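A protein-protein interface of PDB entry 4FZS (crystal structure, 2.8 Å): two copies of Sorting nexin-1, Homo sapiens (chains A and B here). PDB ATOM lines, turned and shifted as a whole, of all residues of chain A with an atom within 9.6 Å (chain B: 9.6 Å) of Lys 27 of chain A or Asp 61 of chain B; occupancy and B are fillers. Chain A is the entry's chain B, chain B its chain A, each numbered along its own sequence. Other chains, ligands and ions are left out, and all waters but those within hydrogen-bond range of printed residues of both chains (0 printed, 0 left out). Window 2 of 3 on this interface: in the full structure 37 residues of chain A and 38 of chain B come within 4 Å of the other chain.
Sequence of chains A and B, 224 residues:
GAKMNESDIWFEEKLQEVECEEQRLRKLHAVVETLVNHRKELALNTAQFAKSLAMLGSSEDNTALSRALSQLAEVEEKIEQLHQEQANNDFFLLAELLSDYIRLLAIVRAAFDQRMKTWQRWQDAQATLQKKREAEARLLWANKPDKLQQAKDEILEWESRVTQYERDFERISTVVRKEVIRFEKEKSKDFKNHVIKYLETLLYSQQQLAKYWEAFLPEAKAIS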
ATOM      1  N   GLU A  19     -17.782 -13.200  19.046  1.00  0.00           N
ATOM      2  CA  GLU A  19     -16.844 -13.034  17.922  1.00  0.00           C
ATOM      3  C   GLU A  19     -16.625 -11.547  17.587  1.00  0.00           C
ATOM      4  O   GLU A  19     -15.496 -11.128  17.297  1.00  0.00           O
ATOM      5  CB  GLU A  19     -17.299 -13.822  16.679  1.00  0.00           C
ATOM      6  CG  GLU A  19     -16.979 -15.301  16.759  1.00  0.00           C
ATOM      7  CD  GLU A  19     -17.457 -16.130  15.588  1.00  0.00           C
ATOM      8  OE1 GLU A  19     -18.689 -16.321  15.466  1.00  0.00           O
ATOM      9  OE2 GLU A  19     -16.599 -16.626  14.822  1.00  0.00           O
ATOM     10  N   CYS A  20     -17.717 -10.755  17.686  1.00  0.00           N
ATOM     11  CA  CYS A  20     -17.756  -9.325  17.408  1.00  0.00           C
ATOM     12  C   CYS A  20     -16.989  -8.534  18.458  1.00  0.00           C
ATOM     13  O   CYS A  20     -16.045  -7.838  18.086  1.00  0.00           O
ATOM     14  CB  CYS A  20     -19.199  -8.846  17.270  1.00  0.00           C
ATOM     15  SG  CYS A  20     -19.365  -7.073  16.964  1.00  0.00           S
ATOM     16  N   GLU A  21     -17.376  -8.656  19.758  1.00  0.00           N
ATOM     17  CA  GLU A  21     -16.709  -8.017  20.899  1.00  0.00           C
ATOM     18  C   GLU A  21     -15.198  -8.316  20.912  1.00  0.00           C
ATOM     19  O   GLU A  21     -14.399  -7.416  21.156  1.00  0.00           O
ATOM     20  CB  GLU A  21     -17.316  -8.503  22.194  1.00  0.00           C
ATOM     21  CG  GLU A  21     -18.697  -7.960  22.431  1.00  0.00           C
ATOM     22  CD  GLU A  21     -18.717  -6.585  23.054  1.00  0.00           C
ATOM     23  OE1 GLU A  21     -19.071  -5.627  22.329  1.00  0.00           O
ATOM     24  OE2 GLU A  21     -18.417  -6.470  24.267  1.00  0.00           O
ATOM     25  N   GLU A  22     -14.808  -9.570  20.604  1.00  0.00           N
ATOM     26  CA  GLU A  22     -13.398  -9.966  20.540  1.00  0.00           C
ATOM     27  C   GLU A  22     -12.657  -9.207  19.442  1.00  0.00           C
ATOM     28  O   GLU A  22     -11.484  -8.903  19.611  1.00  0.00           O
ATOM     29  CB  GLU A  22     -13.242 -11.489  20.349  1.00  0.00           C
ATOM     30  CG  GLU A  22     -11.899 -12.045  20.812  1.00  0.00           C
ATOM     31  CD  GLU A  22     -11.457 -13.327  20.131  1.00  0.00           C
ATOM     32  OE1 GLU A  22     -11.668 -13.446  18.902  1.00  0.00           O
ATOM     33  OE2 GLU A  22     -10.847 -14.186  20.808  1.00  0.00           O
ATOM     34  N   GLN A  23     -13.335  -8.909  18.329  1.00  0.00           N
ATOM     35  CA  GLN A  23     -12.738  -8.216  17.194  1.00  0.00           C
ATOM     36  C   GLN A  23     -12.627  -6.730  17.521  1.00  0.00           C
ATOM     37  O   GLN A  23     -11.627  -6.098  17.175  1.00  0.00           O
ATOM     38  CB  GLN A  23     -13.582  -8.456  15.934  1.00  0.00           C
ATOM     39  CG  GLN A  23     -12.781  -8.395  14.634  1.00  0.00           C
ATOM     40  CD  GLN A  23     -13.579  -8.924  13.460  1.00  0.00           C
ATOM     41  OE1 GLN A  23     -14.662  -8.418  13.120  1.00  0.00           O
ATOM     42  NE2 GLN A  23     -13.054  -9.951  12.805  1.00  0.00           N
ATOM     43  N   ARG A  24     -13.651  -6.196  18.227  1.00  0.00           N
ATOM     44  CA  ARG A  24     -13.763  -4.812  18.662  1.00  0.00           C
ATOM     45  C   ARG A  24     -12.759  -4.497  19.776  1.00  0.00           C
ATOM     46  O   ARG A  24     -12.061  -3.481  19.694  1.00  0.00           O
ATOM     47  CB  ARG A  24     -15.207  -4.527  19.106  1.00  0.00           C
ATOM     48  CG  ARG A  24     -15.467  -3.089  19.515  1.00  0.00           C
ATOM     49  CD  ARG A  24     -16.897  -2.877  19.954  1.00  0.00           C
ATOM     50  NE  ARG A  24     -17.818  -2.714  18.826  1.00  0.00           N
ATOM     51  CZ  ARG A  24     -18.806  -3.547  18.519  1.00  0.00           C
ATOM     52  NH1 ARG A  24     -19.025  -4.631  19.254  1.00  0.00           N
ATOM     53  NH2 ARG A  24     -19.594  -3.293  17.487  1.00  0.00           N
ATOM     54  N   LEU A  25     -12.682  -5.358  20.802  1.00  0.00           N
ATOM     55  CA  LEU A  25     -11.797  -5.142  21.942  1.00  0.00           C
ATOM     56  C   LEU A  25     -10.343  -5.313  21.656  1.00  0.00           C
ATOM     57  O   LEU A  25      -9.529  -4.603  22.252  1.00  0.00           O
ATOM     58  CB  LEU A  25     -12.252  -5.848  23.224  1.00  0.00           C
ATOM     59  CG  LEU A  25     -13.607  -5.386  23.789  1.00  0.00           C
ATOM     60  CD1 LEU A  25     -13.685  -5.596  25.253  1.00  0.00           C
ATOM     61  CD2 LEU A  25     -13.852  -3.938  23.497  1.00  0.00           C
ATOM     62  N   ARG A  26     -10.010  -6.173  20.681  1.00  0.00           N
ATOM     63  CA  ARG A  26      -8.627  -6.359  20.242  1.00  0.00           C
ATOM     64  C   ARG A  26      -8.118  -5.082  19.584  1.00  0.00           C
ATOM     65  O   ARG A  26      -6.957  -4.716  19.798  1.00  0.00           O
ATOM     66  CB  ARG A  26      -8.478  -7.565  19.303  1.00  0.00           C
ATOM     67  CG  ARG A  26      -8.284  -8.844  20.080  1.00  0.00           C
ATOM     68  CD  ARG A  26      -7.915 -10.018  19.205  1.00  0.00           C
ATOM     69  NE  ARG A  26      -8.004 -11.238  20.004  1.00  0.00           N
ATOM     70  CZ  ARG A  26      -6.978 -11.822  20.618  1.00  0.00           C
ATOM     71  NH1 ARG A  26      -5.747 -11.337  20.480  1.00  0.00           N
ATOM     72  NH2 ARG A  26      -7.171 -12.909  21.354  1.00  0.00           N
ATOM     73  N   LYS A  27      -9.014  -4.383  18.825  1.00  0.00           N
ATOM     74  CA  LYS A  27      -8.740  -3.105  18.163  1.00  0.00           C
ATOM     75  C   LYS A  27      -8.479  -2.039  19.230  1.00  0.00           C
ATOM     76  O   LYS A  27      -7.499  -1.296  19.127  1.00  0.00           O
ATOM     77  CB  LYS A  27      -9.917  -2.671  17.255  1.00  0.00           C
ATOM     78  CG  LYS A  27      -9.871  -3.242  15.843  1.00  0.00           C
ATOM     79  CD  LYS A  27     -10.945  -2.626  14.938  1.00  0.00           C
ATOM     80  CE  LYS A  27     -12.308  -3.281  15.168  1.00  0.00           C
ATOM     81  NZ  LYS A  27     -13.363  -2.755  14.256  1.00  0.00           N
ATOM     82  N   LEU A  28      -9.344  -1.989  20.273  1.00  0.00           N
ATOM     83  CA  LEU A  28      -9.219  -1.038  21.365  1.00  0.00           C
ATOM     84  C   LEU A  28      -7.948  -1.301  22.128  1.00  0.00           C
ATOM     85  O   LEU A  28      -7.243  -0.355  22.456  1.00  0.00           O
ATOM     86  CB  LEU A  28     -10.433  -1.109  22.296  1.00  0.00           C
ATOM     87  CG  LEU A  28     -10.569   0.027  23.327  1.00  0.00           C
ATOM     88  CD1 LEU A  28     -10.844   1.346  22.650  1.00  0.00           C
ATOM     89  CD2 LEU A  28     -11.653  -0.284  24.342  1.00  0.00           C
ATOM     90  N   HIS A  29      -7.629  -2.584  22.374  1.00  0.00           N
ATOM     91  CA  HIS A  29      -6.433  -3.011  23.105  1.00  0.00           C
ATOM     92  C   HIS A  29      -5.197  -2.437  22.471  1.00  0.00           C
ATOM     93  O   HIS A  29      -4.373  -1.896  23.195  1.00  0.00           O
ATOM     94  CB  HIS A  29      -6.349  -4.536  23.141  1.00  0.00           C
ATOM     95  CG  HIS A  29      -5.256  -5.074  24.009  1.00  0.00           C
ATOM     96  ND1 HIS A  29      -5.348  -5.039  25.392  1.00  0.00           N
ATOM     97  CD2 HIS A  29      -4.095  -5.676  23.659  1.00  0.00           C
ATOM     98  CE1 HIS A  29      -4.238  -5.607  25.834  1.00  0.00           C
ATOM     99  NE2 HIS A  29      -3.456  -6.007  24.825  1.00  0.00           N
ATOM    100  N   ALA A  30      -5.094  -2.506  21.116  1.00  0.00           N
ATOM    101  CA  ALA A  30      -3.979  -1.977  20.319  1.00  0.00           C
ATOM    102  C   ALA A  30      -3.804  -0.463  20.549  1.00  0.00           C
ATOM    103  O   ALA A  30      -2.663   0.015  20.611  1.00  0.00           O
ATOM    104  CB  ALA A  30      -4.180  -2.289  18.846  1.00  0.00           C
ATOM    105  N   VAL A  31      -4.930   0.275  20.756  1.00  0.00           N
ATOM    106  CA  VAL A  31      -4.863   1.697  21.101  1.00  0.00           C
ATOM    107  C   VAL A  31      -4.384   1.861  22.548  1.00  0.00           C
ATOM    108  O   VAL A  31      -3.395   2.561  22.778  1.00  0.00           O
ATOM    109  CB  VAL A  31      -6.086   2.597  20.757  1.00  0.00           C
ATOM    110  CG1 VAL A  31      -6.702   2.291  19.408  1.00  0.00           C
ATOM    111  CG2 VAL A  31      -7.116   2.761  21.868  1.00  0.00           C
ATOM    112  N   VAL A  32      -5.044   1.180  23.508  1.00  0.00           N
ATOM    113  CA  VAL A  32      -4.688   1.252  24.923  1.00  0.00           C
ATOM    114  C   VAL A  32      -3.220   0.850  25.133  1.00  0.00           C
ATOM    115  O   VAL A  32      -2.492   1.574  25.815  1.00  0.00           O
ATOM    116  CB  VAL A  32      -5.690   0.484  25.823  1.00  0.00           C
ATOM    117  CG1 VAL A  32      -5.210   0.401  27.262  1.00  0.00           C
ATOM    118  CG2 VAL A  32      -7.059   1.130  25.770  1.00  0.00           C
ATOM    119  N   GLU A  33      -2.776  -0.241  24.479  1.00  0.00           N
ATOM    120  CA  GLU A  33      -1.391  -0.688  24.585  1.00  0.00           C
ATOM    121  C   GLU A  33      -0.363   0.319  24.081  1.00  0.00           C
ATOM    122  O   GLU A  33       0.702   0.392  24.688  1.00  0.00           O
ATOM    123  CB  GLU A  33      -1.163  -2.107  24.047  1.00  0.00           C
ATOM    124  CG  GLU A  33      -1.440  -3.182  25.088  1.00  0.00           C
ATOM    125  CD  GLU A  33      -0.306  -3.505  26.051  1.00  0.00           C
ATOM    126  OE1 GLU A  33       0.727  -4.047  25.591  1.00  0.00           O
ATOM    127  OE2 GLU A  33      -0.470  -3.262  27.270  1.00  0.00           O
ATOM    128  N   THR A  34      -0.677   1.139  23.051  1.00  0.00           N
ATOM    129  CA  THR A  34       0.321   2.128  22.654  1.00  0.00           C
ATOM    130  C   THR A  34       0.390   3.275  23.648  1.00  0.00           C
ATOM    131  O   THR A  34       1.479   3.812  23.889  1.00  0.00           O
ATOM    132  CB  THR A  34       0.339   2.499  21.164  1.00  0.00           C
ATOM    133  OG1 THR A  34      -0.635   3.494  20.880  1.00  0.00           O
ATOM    134  CG2 THR A  34       0.210   1.294  20.233  1.00  0.00           C
ATOM    135  N   LEU A  98      -9.045  -4.758  30.614  1.00  0.00           N
ATOM    136  CA  LEU A  98      -9.204  -4.965  29.183  1.00  0.00           C
ATOM    137  C   LEU A  98      -8.340  -6.129  28.691  1.00  0.00           C
ATOM    138  O   LEU A  98      -8.830  -6.962  27.941  1.00  0.00           O
ATOM    139  CB  LEU A  98      -8.870  -3.653  28.404  1.00  0.00           C
ATOM    140  CG  LEU A  98      -8.961  -3.732  26.865  1.00  0.00           C
ATOM    141  CD1 LEU A  98     -10.383  -3.943  26.411  1.00  0.00           C
ATOM    142  CD2 LEU A  98      -8.377  -2.510  26.211  1.00  0.00           C
ATOM    143  N   ILE A 102      -9.965  -9.676  27.234  1.00  0.00           N
ATOM    144  CA  ILE A 102      -9.586 -10.128  25.877  1.00  0.00           C
ATOM    145  C   ILE A 102      -9.164 -11.592  25.902  1.00  0.00           C
ATOM    146  O   ILE A 102      -9.599 -12.350  25.033  1.00  0.00           O
ATOM    147  CB  ILE A 102      -8.543  -9.183  25.186  1.00  0.00           C
ATOM    148  CG1 ILE A 102      -9.253  -8.095  24.398  1.00  0.00           C
ATOM    149  CG2 ILE A 102      -7.584  -9.915  24.257  1.00  0.00           C
ATOM    150  CD1 ILE A 102      -8.657  -6.810  24.514  1.00  0.00           C
ATOM    151  N   LEU A 105     -12.273 -13.852  26.423  1.00  0.00           N
ATOM    152  CA  LEU A 105     -13.005 -13.993  25.156  1.00  0.00           C
ATOM    153  C   LEU A 105     -12.376 -15.045  24.270  1.00  0.00           C
ATOM    154  O   LEU A 105     -13.106 -15.784  23.608  1.00  0.00           O
ATOM    155  CB  LEU A 105     -13.142 -12.669  24.401  1.00  0.00           C
ATOM    156  CG  LEU A 105     -14.012 -11.543  25.056  1.00  0.00           C
ATOM    157  CD1 LEU A 105     -14.012 -10.280  24.184  1.00  0.00           C
ATOM    158  CD2 LEU A 105     -15.445 -11.982  25.298  1.00  0.00           C
ATOM    159  N   SER A 188     -18.061  -3.434  25.658  1.00  0.00           N
ATOM    160  CA  SER A 188     -16.984  -2.825  24.887  1.00  0.00           C
ATOM    161  C   SER A 188     -17.151  -1.338  24.678  1.00  0.00           C
ATOM    162  O   SER A 188     -16.173  -0.601  24.774  1.00  0.00           O
ATOM    163  CB  SER A 188     -16.884  -3.491  23.523  1.00  0.00           C
ATOM    164  OG  SER A 188     -18.029  -3.194  22.746  1.00  0.00           O
ATOM    165  N   LYS A 189     -18.380  -0.904  24.330  1.00  0.00           N
ATOM    166  CA  LYS A 189     -18.714   0.489  24.050  1.00  0.00           C
ATOM    167  C   LYS A 189     -18.877   1.331  25.330  1.00  0.00           C
ATOM    168  O   LYS A 189     -19.344   2.466  25.254  1.00  0.00           O
ATOM    169  CB  LYS A 189     -19.919   0.583  23.086  1.00  0.00           C
ATOM    170  CG  LYS A 189     -19.598   0.115  21.655  1.00  0.00           C
ATOM    171  CD  LYS A 189     -20.804   0.165  20.739  1.00  0.00           C
ATOM    172  CE  LYS A 189     -20.502  -0.271  19.313  1.00  0.00           C
ATOM    173  NZ  LYS A 189     -21.745  -0.495  18.504  1.00  0.00           N
ATOM    174  N   LYS A 192     -14.623   1.966  25.693  1.00  0.00           N
ATOM    175  CA  LYS A 192     -14.277   2.897  24.612  1.00  0.00           C
ATOM    176  C   LYS A 192     -14.446   4.359  24.972  1.00  0.00           C
ATOM    177  O   LYS A 192     -13.620   5.175  24.563  1.00  0.00           O
ATOM    178  CB  LYS A 192     -15.060   2.569  23.328  1.00  0.00           C
ATOM    179  CG  LYS A 192     -14.291   2.865  22.039  1.00  0.00           C
ATOM    180  CD  LYS A 192     -15.082   2.453  20.791  1.00  0.00           C
ATOM    181  CE  LYS A 192     -14.265   1.714  19.750  1.00  0.00           C
ATOM    182  NZ  LYS A 192     -15.125   1.132  18.682  1.00  0.00           N
ATOM    183  N   VAL A 195     -11.612   5.477  27.271  1.00  0.00           N
ATOM    184  CA  VAL A 195     -10.425   5.647  26.437  1.00  0.00           C
ATOM    185  C   VAL A 195     -10.508   7.007  25.743  1.00  0.00           C
ATOM    186  O   VAL A 195      -9.535   7.750  25.764  1.00  0.00           O
ATOM    187  CB  VAL A 195     -10.269   4.469  25.448  1.00  0.00           C
ATOM    188  CG1 VAL A 195      -9.128   4.702  24.474  1.00  0.00           C
ATOM    189  CG2 VAL A 195     -10.079   3.155  26.195  1.00  0.00           C
ATOM    190  N   ILE A 196     -11.683   7.366  25.197  1.00  0.00           N
ATOM    191  CA  ILE A 196     -11.880   8.665  24.541  1.00  0.00           C
ATOM    192  C   ILE A 196     -11.637   9.820  25.546  1.00  0.00           C
ATOM    193  O   ILE A 196     -10.863  10.736  25.245  1.00  0.00           O
ATOM    194  CB  ILE A 196     -13.228   8.737  23.811  1.00  0.00           C
ATOM    195  CG1 ILE A 196     -13.243   7.732  22.641  1.00  0.00           C
ATOM    196  CG2 ILE A 196     -13.499  10.162  23.313  1.00  0.00           C
ATOM    197  CD1 ILE A 196     -14.631   7.277  22.136  1.00  0.00           C
ATOM    198  N   MET B  55      -1.692   5.915  12.301  1.00  0.00           N
ATOM    199  CA  MET B  55      -2.066   4.644  11.707  1.00  0.00           C
ATOM    200  C   MET B  55      -3.319   4.122  12.421  1.00  0.00           C
ATOM    201  O   MET B  55      -4.307   3.807  11.756  1.00  0.00           O
ATOM    202  CB  MET B  55      -0.893   3.647  11.759  1.00  0.00           C
ATOM    203  CG  MET B  55      -1.258   2.247  11.280  1.00  0.00           C
ATOM    204  SD  MET B  55      -1.843   1.148  12.626  1.00  0.00           S
ATOM    205  CE  MET B  55      -3.286   0.332  11.810  1.00  0.00           C
ATOM    206  N   LEU B  56      -3.289   4.056  13.764  1.00  0.00           N
ATOM    207  CA  LEU B  56      -4.421   3.587  14.579  1.00  0.00           C
ATOM    208  C   LEU B  56      -5.673   4.459  14.366  1.00  0.00           C
ATOM    209  O   LEU B  56      -6.797   3.943  14.337  1.00  0.00           O
ATOM    210  CB  LEU B  56      -4.056   3.580  16.077  1.00  0.00           C
ATOM    211  CG  LEU B  56      -3.132   2.482  16.566  1.00  0.00           C
ATOM    212  CD1 LEU B  56      -2.368   2.945  17.790  1.00  0.00           C
ATOM    213  CD2 LEU B  56      -3.903   1.221  16.890  1.00  0.00           C
ATOM    214  N   GLY B  57      -5.458   5.769  14.259  1.00  0.00           N
ATOM    215  CA  GLY B  57      -6.510   6.756  14.047  1.00  0.00           C
ATOM    216  C   GLY B  57      -7.119   6.643  12.669  1.00  0.00           C
ATOM    217  O   GLY B  57      -8.318   6.878  12.491  1.00  0.00           O
ATOM    218  N   SER B  58      -6.283   6.265  11.688  1.00  0.00           N
ATOM    219  CA  SER B  58      -6.707   6.071  10.309  1.00  0.00           C
ATOM    220  C   SER B  58      -7.563   4.811  10.206  1.00  0.00           C
ATOM    221  O   SER B  58      -8.561   4.817   9.483  1.00  0.00           O
ATOM    222  CB  SER B  58      -5.501   5.985   9.379  1.00  0.00           C
ATOM    223  OG  SER B  58      -5.917   5.891   8.028  1.00  0.00           O
ATOM    224  N   SER B  59      -7.197   3.751  10.951  1.00  0.00           N
ATOM    225  CA  SER B  59      -7.918   2.487  10.936  1.00  0.00           C
ATOM    226  C   SER B  59      -9.089   2.362  11.968  1.00  0.00           C
ATOM    227  O   SER B  59      -9.609   1.267  12.186  1.00  0.00           O
ATOM    228  CB  SER B  59      -6.920   1.333  11.008  1.00  0.00           C
ATOM    229  OG  SER B  59      -6.464   1.095  12.324  1.00  0.00           O
ATOM    230  N   GLU B  60      -9.525   3.491  12.559  1.00  0.00           N
ATOM    231  CA  GLU B  60     -10.608   3.536  13.556  1.00  0.00           C
ATOM    232  C   GLU B  60     -11.956   3.913  12.946  1.00  0.00           C
ATOM    233  O   GLU B  60     -12.066   4.922  12.235  1.00  0.00           O
ATOM    234  CB  GLU B  60     -10.254   4.500  14.711  1.00  0.00           C
ATOM    235  CG  GLU B  60     -11.283   4.579  15.840  1.00  0.00           C
ATOM    236  CD  GLU B  60     -11.630   3.270  16.519  1.00  0.00           C
ATOM    237  OE1 GLU B  60     -12.831   3.025  16.778  1.00  0.00           O
ATOM    238  OE2 GLU B  60     -10.693   2.488  16.796  1.00  0.00           O
ATOM    239  N   ASP B  61     -12.986   3.131  13.285  1.00  0.00           N
ATOM    240  CA  ASP B  61     -14.349   3.340  12.811  1.00  0.00           C
ATOM    241  C   ASP B  61     -15.178   4.314  13.639  1.00  0.00           C
ATOM    242  O   ASP B  61     -16.125   4.916  13.107  1.00  0.00           O
ATOM    243  CB  ASP B  61     -15.060   2.012  12.623  1.00  0.00           C
ATOM    244  CG  ASP B  61     -14.519   1.224  11.461  1.00  0.00           C
ATOM    245  OD1 ASP B  61     -14.150   1.847  10.455  1.00  0.00           O
ATOM    246  OD2 ASP B  61     -14.470  -0.029  11.559  1.00  0.00           O
ATOM    247  N   ASN B  62     -14.839   4.481  14.929  1.00  0.00           N
ATOM    248  CA  ASN B  62     -15.512   5.442  15.792  1.00  0.00           C
ATOM    249  C   ASN B  62     -14.924   6.844  15.508  1.00  0.00           C
ATOM    250  O   ASN B  62     -13.734   7.069  15.716  1.00  0.00           O
ATOM    251  CB  ASN B  62     -15.349   5.049  17.244  1.00  0.00           C
ATOM    252  CG  ASN B  62     -15.939   6.040  18.206  1.00  0.00           C
ATOM    253  OD1 ASN B  62     -15.465   7.163  18.362  1.00  0.00           O
ATOM    254  ND2 ASN B  62     -16.999   5.660  18.867  1.00  0.00           N
ATOM    255  N   THR B  63     -15.766   7.773  15.040  1.00  0.00           N
ATOM    256  CA  THR B  63     -15.381   9.133  14.667  1.00  0.00           C
ATOM    257  C   THR B  63     -14.706   9.945  15.781  1.00  0.00           C
ATOM    258  O   THR B  63     -13.721  10.636  15.515  1.00  0.00           O
ATOM    259  CB  THR B  63     -16.566   9.814  13.992  1.00  0.00           C
ATOM    260  OG1 THR B  63     -17.038   8.924  12.971  1.00  0.00           O
ATOM    261  CG2 THR B  63     -16.203  11.166  13.376  1.00  0.00           C
ATOM    262  N   ALA B  64     -15.232   9.851  17.016  1.00  0.00           N
ATOM    263  CA  ALA B  64     -14.689  10.551  18.174  1.00  0.00           C
ATOM    264  C   ALA B  64     -13.284  10.012  18.499  1.00  0.00           C
ATOM    265  O   ALA B  64     -12.340  10.803  18.619  1.00  0.00           O
ATOM    266  CB  ALA B  64     -15.619  10.384  19.360  1.00  0.00           C
ATOM    267  N   LEU B  65     -13.138   8.670  18.567  1.00  0.00           N
ATOM    268  CA  LEU B  65     -11.865   8.012  18.826  1.00  0.00           C
ATOM    269  C   LEU B  65     -10.887   8.295  17.697  1.00  0.00           C
ATOM    270  O   LEU B  65      -9.725   8.571  17.980  1.00  0.00           O
ATOM    271  CB  LEU B  65     -12.052   6.490  18.963  1.00  0.00           C
ATOM    272  CG  LEU B  65     -11.358   5.774  20.117  1.00  0.00           C
ATOM    273  CD1 LEU B  65     -11.478   4.319  19.957  1.00  0.00           C
ATOM    274  CD2 LEU B  65      -9.904   6.081  20.207  1.00  0.00           C
ATOM    275  N   SER B  66     -11.346   8.213  16.426  1.00  0.00           N
ATOM    276  CA  SER B  66     -10.509   8.449  15.252  1.00  0.00           C
ATOM    277  C   SER B  66      -9.897   9.841  15.284  1.00  0.00           C
ATOM    278  O   SER B  66      -8.677   9.941  15.134  1.00  0.00           O
ATOM    279  CB  SER B  66     -11.283   8.238  13.955  1.00  0.00           C
ATOM    280  OG  SER B  66     -10.440   8.490  12.841  1.00  0.00           O
ATOM    281  N   ARG B  67     -10.729  10.902  15.514  1.00  0.00           N
ATOM    282  CA  ARG B  67     -10.297  12.298  15.583  1.00  0.00           C
ATOM    283  C   ARG B  67      -9.308  12.497  16.705  1.00  0.00           C
ATOM    284  O   ARG B  67      -8.270  13.119  16.471  1.00  0.00           O
ATOM    285  CB  ARG B  67     -11.484  13.273  15.714  1.00  0.00           C
ATOM    286  CG  ARG B  67     -11.866  13.901  14.381  1.00  0.00           C
ATOM    287  CD  ARG B  67     -13.145  14.719  14.393  1.00  0.00           C
ATOM    288  NE  ARG B  67     -12.996  15.904  13.535  1.00  0.00           N
ATOM    289  CZ  ARG B  67     -14.001  16.636  13.048  1.00  0.00           C
ATOM    290  NH1 ARG B  67     -15.262  16.311  13.314  1.00  0.00           N
ATOM    291  NH2 ARG B  67     -13.751  17.694  12.287  1.00  0.00           N
ATOM    292  N   LEU B  69      -7.268  10.339  18.204  1.00  0.00           N
ATOM    293  CA  LEU B  69      -5.980   9.711  17.873  1.00  0.00           C
ATOM    294  C   LEU B  69      -5.232  10.517  16.838  1.00  0.00           C
ATOM    295  O   LEU B  69      -4.043  10.763  17.022  1.00  0.00           O
ATOM    296  CB  LEU B  69      -6.126   8.258  17.404  1.00  0.00           C
ATOM    297  CG  LEU B  69      -6.655   7.218  18.409  1.00  0.00           C
ATOM    298  CD1 LEU B  69      -7.340   6.071  17.691  1.00  0.00           C
ATOM    299  CD2 LEU B  69      -5.532   6.671  19.278  1.00  0.00           C
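Of the printed residues of chain B, Lys 27 of chain A touches Asp 61. No residue of chain B comes within 4 Å of Ala 30 of chain A. Of the printed residues of chain B, Val 31 of chain A touches Leu 56 (3.9 Å). Printed residues of chain B within 4 Å of Thr 34 of chain A: Leu 56 (3.6 Å). Ile 102 of chain A touches none of the printed residues of chain B. Of the printed residues of chain B, Ile 196 of chain A touches Asn 62 (3.9 Å) and Leu 65 (3.7 Å). Of chain A, only Lys 192 (3.5 Å) comes within 4 Å of Glu 60 of chain B. Printed residues of chain A within 4 Å of Asp 61 of chain B: Lys 27. Of the printed residues of chain A, Asn 62 of chain B touches Ile 196 (3.9 Å). Of the printed residues of chain A, Leu 65 of chain B touches Lys 192 and Ile 196. Leu 69 of chain B touches none of the printed residues of chain A. The nearest printed residue of chain A that does not touch Asp 61 of chain B is Lys 192 of chain A (6.0 Å).
Of the 14 printed residues of chain B, 5 touch a printed residue of chain A. Hydrophobic or aromatic side chains of chain B that line the printed part of chain A: Leu 56 and Leu 65. Along chain A the printed residues that touch a printed residue of chain B span positions 27 to 196. Among the printed residues, Asp or Glu carboxylates within 4 Å of a Lys or Arg side-chain nitrogen of the other chain: Lys 27 of chain A with Asp 61 of chain B and Lys 192 of chain A with Glu 60 of chain B.
OE1 of Glu 60 of chain B lies within hydrogen-bond range of N of Asn 62 of chain B. The side-chain amide oxygen (OD1) of Asn 62 of chain B is in hydrogen-bond range of the backbone NH (N) of Leu 65 of chain B (2.8 Å). The side-chain amide oxygen of Asn 62 of chain B lies within hydrogen-bond range of the backbone NH of Ala 64 of chain B. O of Val 31 of chain A is in hydrogen-bond range of OG1 of Thr 34 of chain A (3.5 Å).
No position is printed for both chains. Of the 7 pairs that touch across the chains among the printed residues, none has its exchanged pair printed and touching as well.
Leu 56 of chain B touches Val 31 of chain A. Thr 34 of chain A touches Leu 56 of chain B. Lys 192 of chain A touches Leu 65 of chain B. CD1 of Ile 196 of chain A touches OD1 of Asn 62 of chain B, at 3.9 Å. Ile 196 of chain A touches Leu 65 of chain B (CG1 to CG, 3.7 Å).
The side-chain carboxylate of Glu 60 of chain B lies within salt-bridge range of the side-chain amino group of Lys 192 of chain A (3.5 Å). NZ of Lys 27 of chain A is in salt-bridge range of OD2 of Asp 61 of chain B (3.99 Å).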
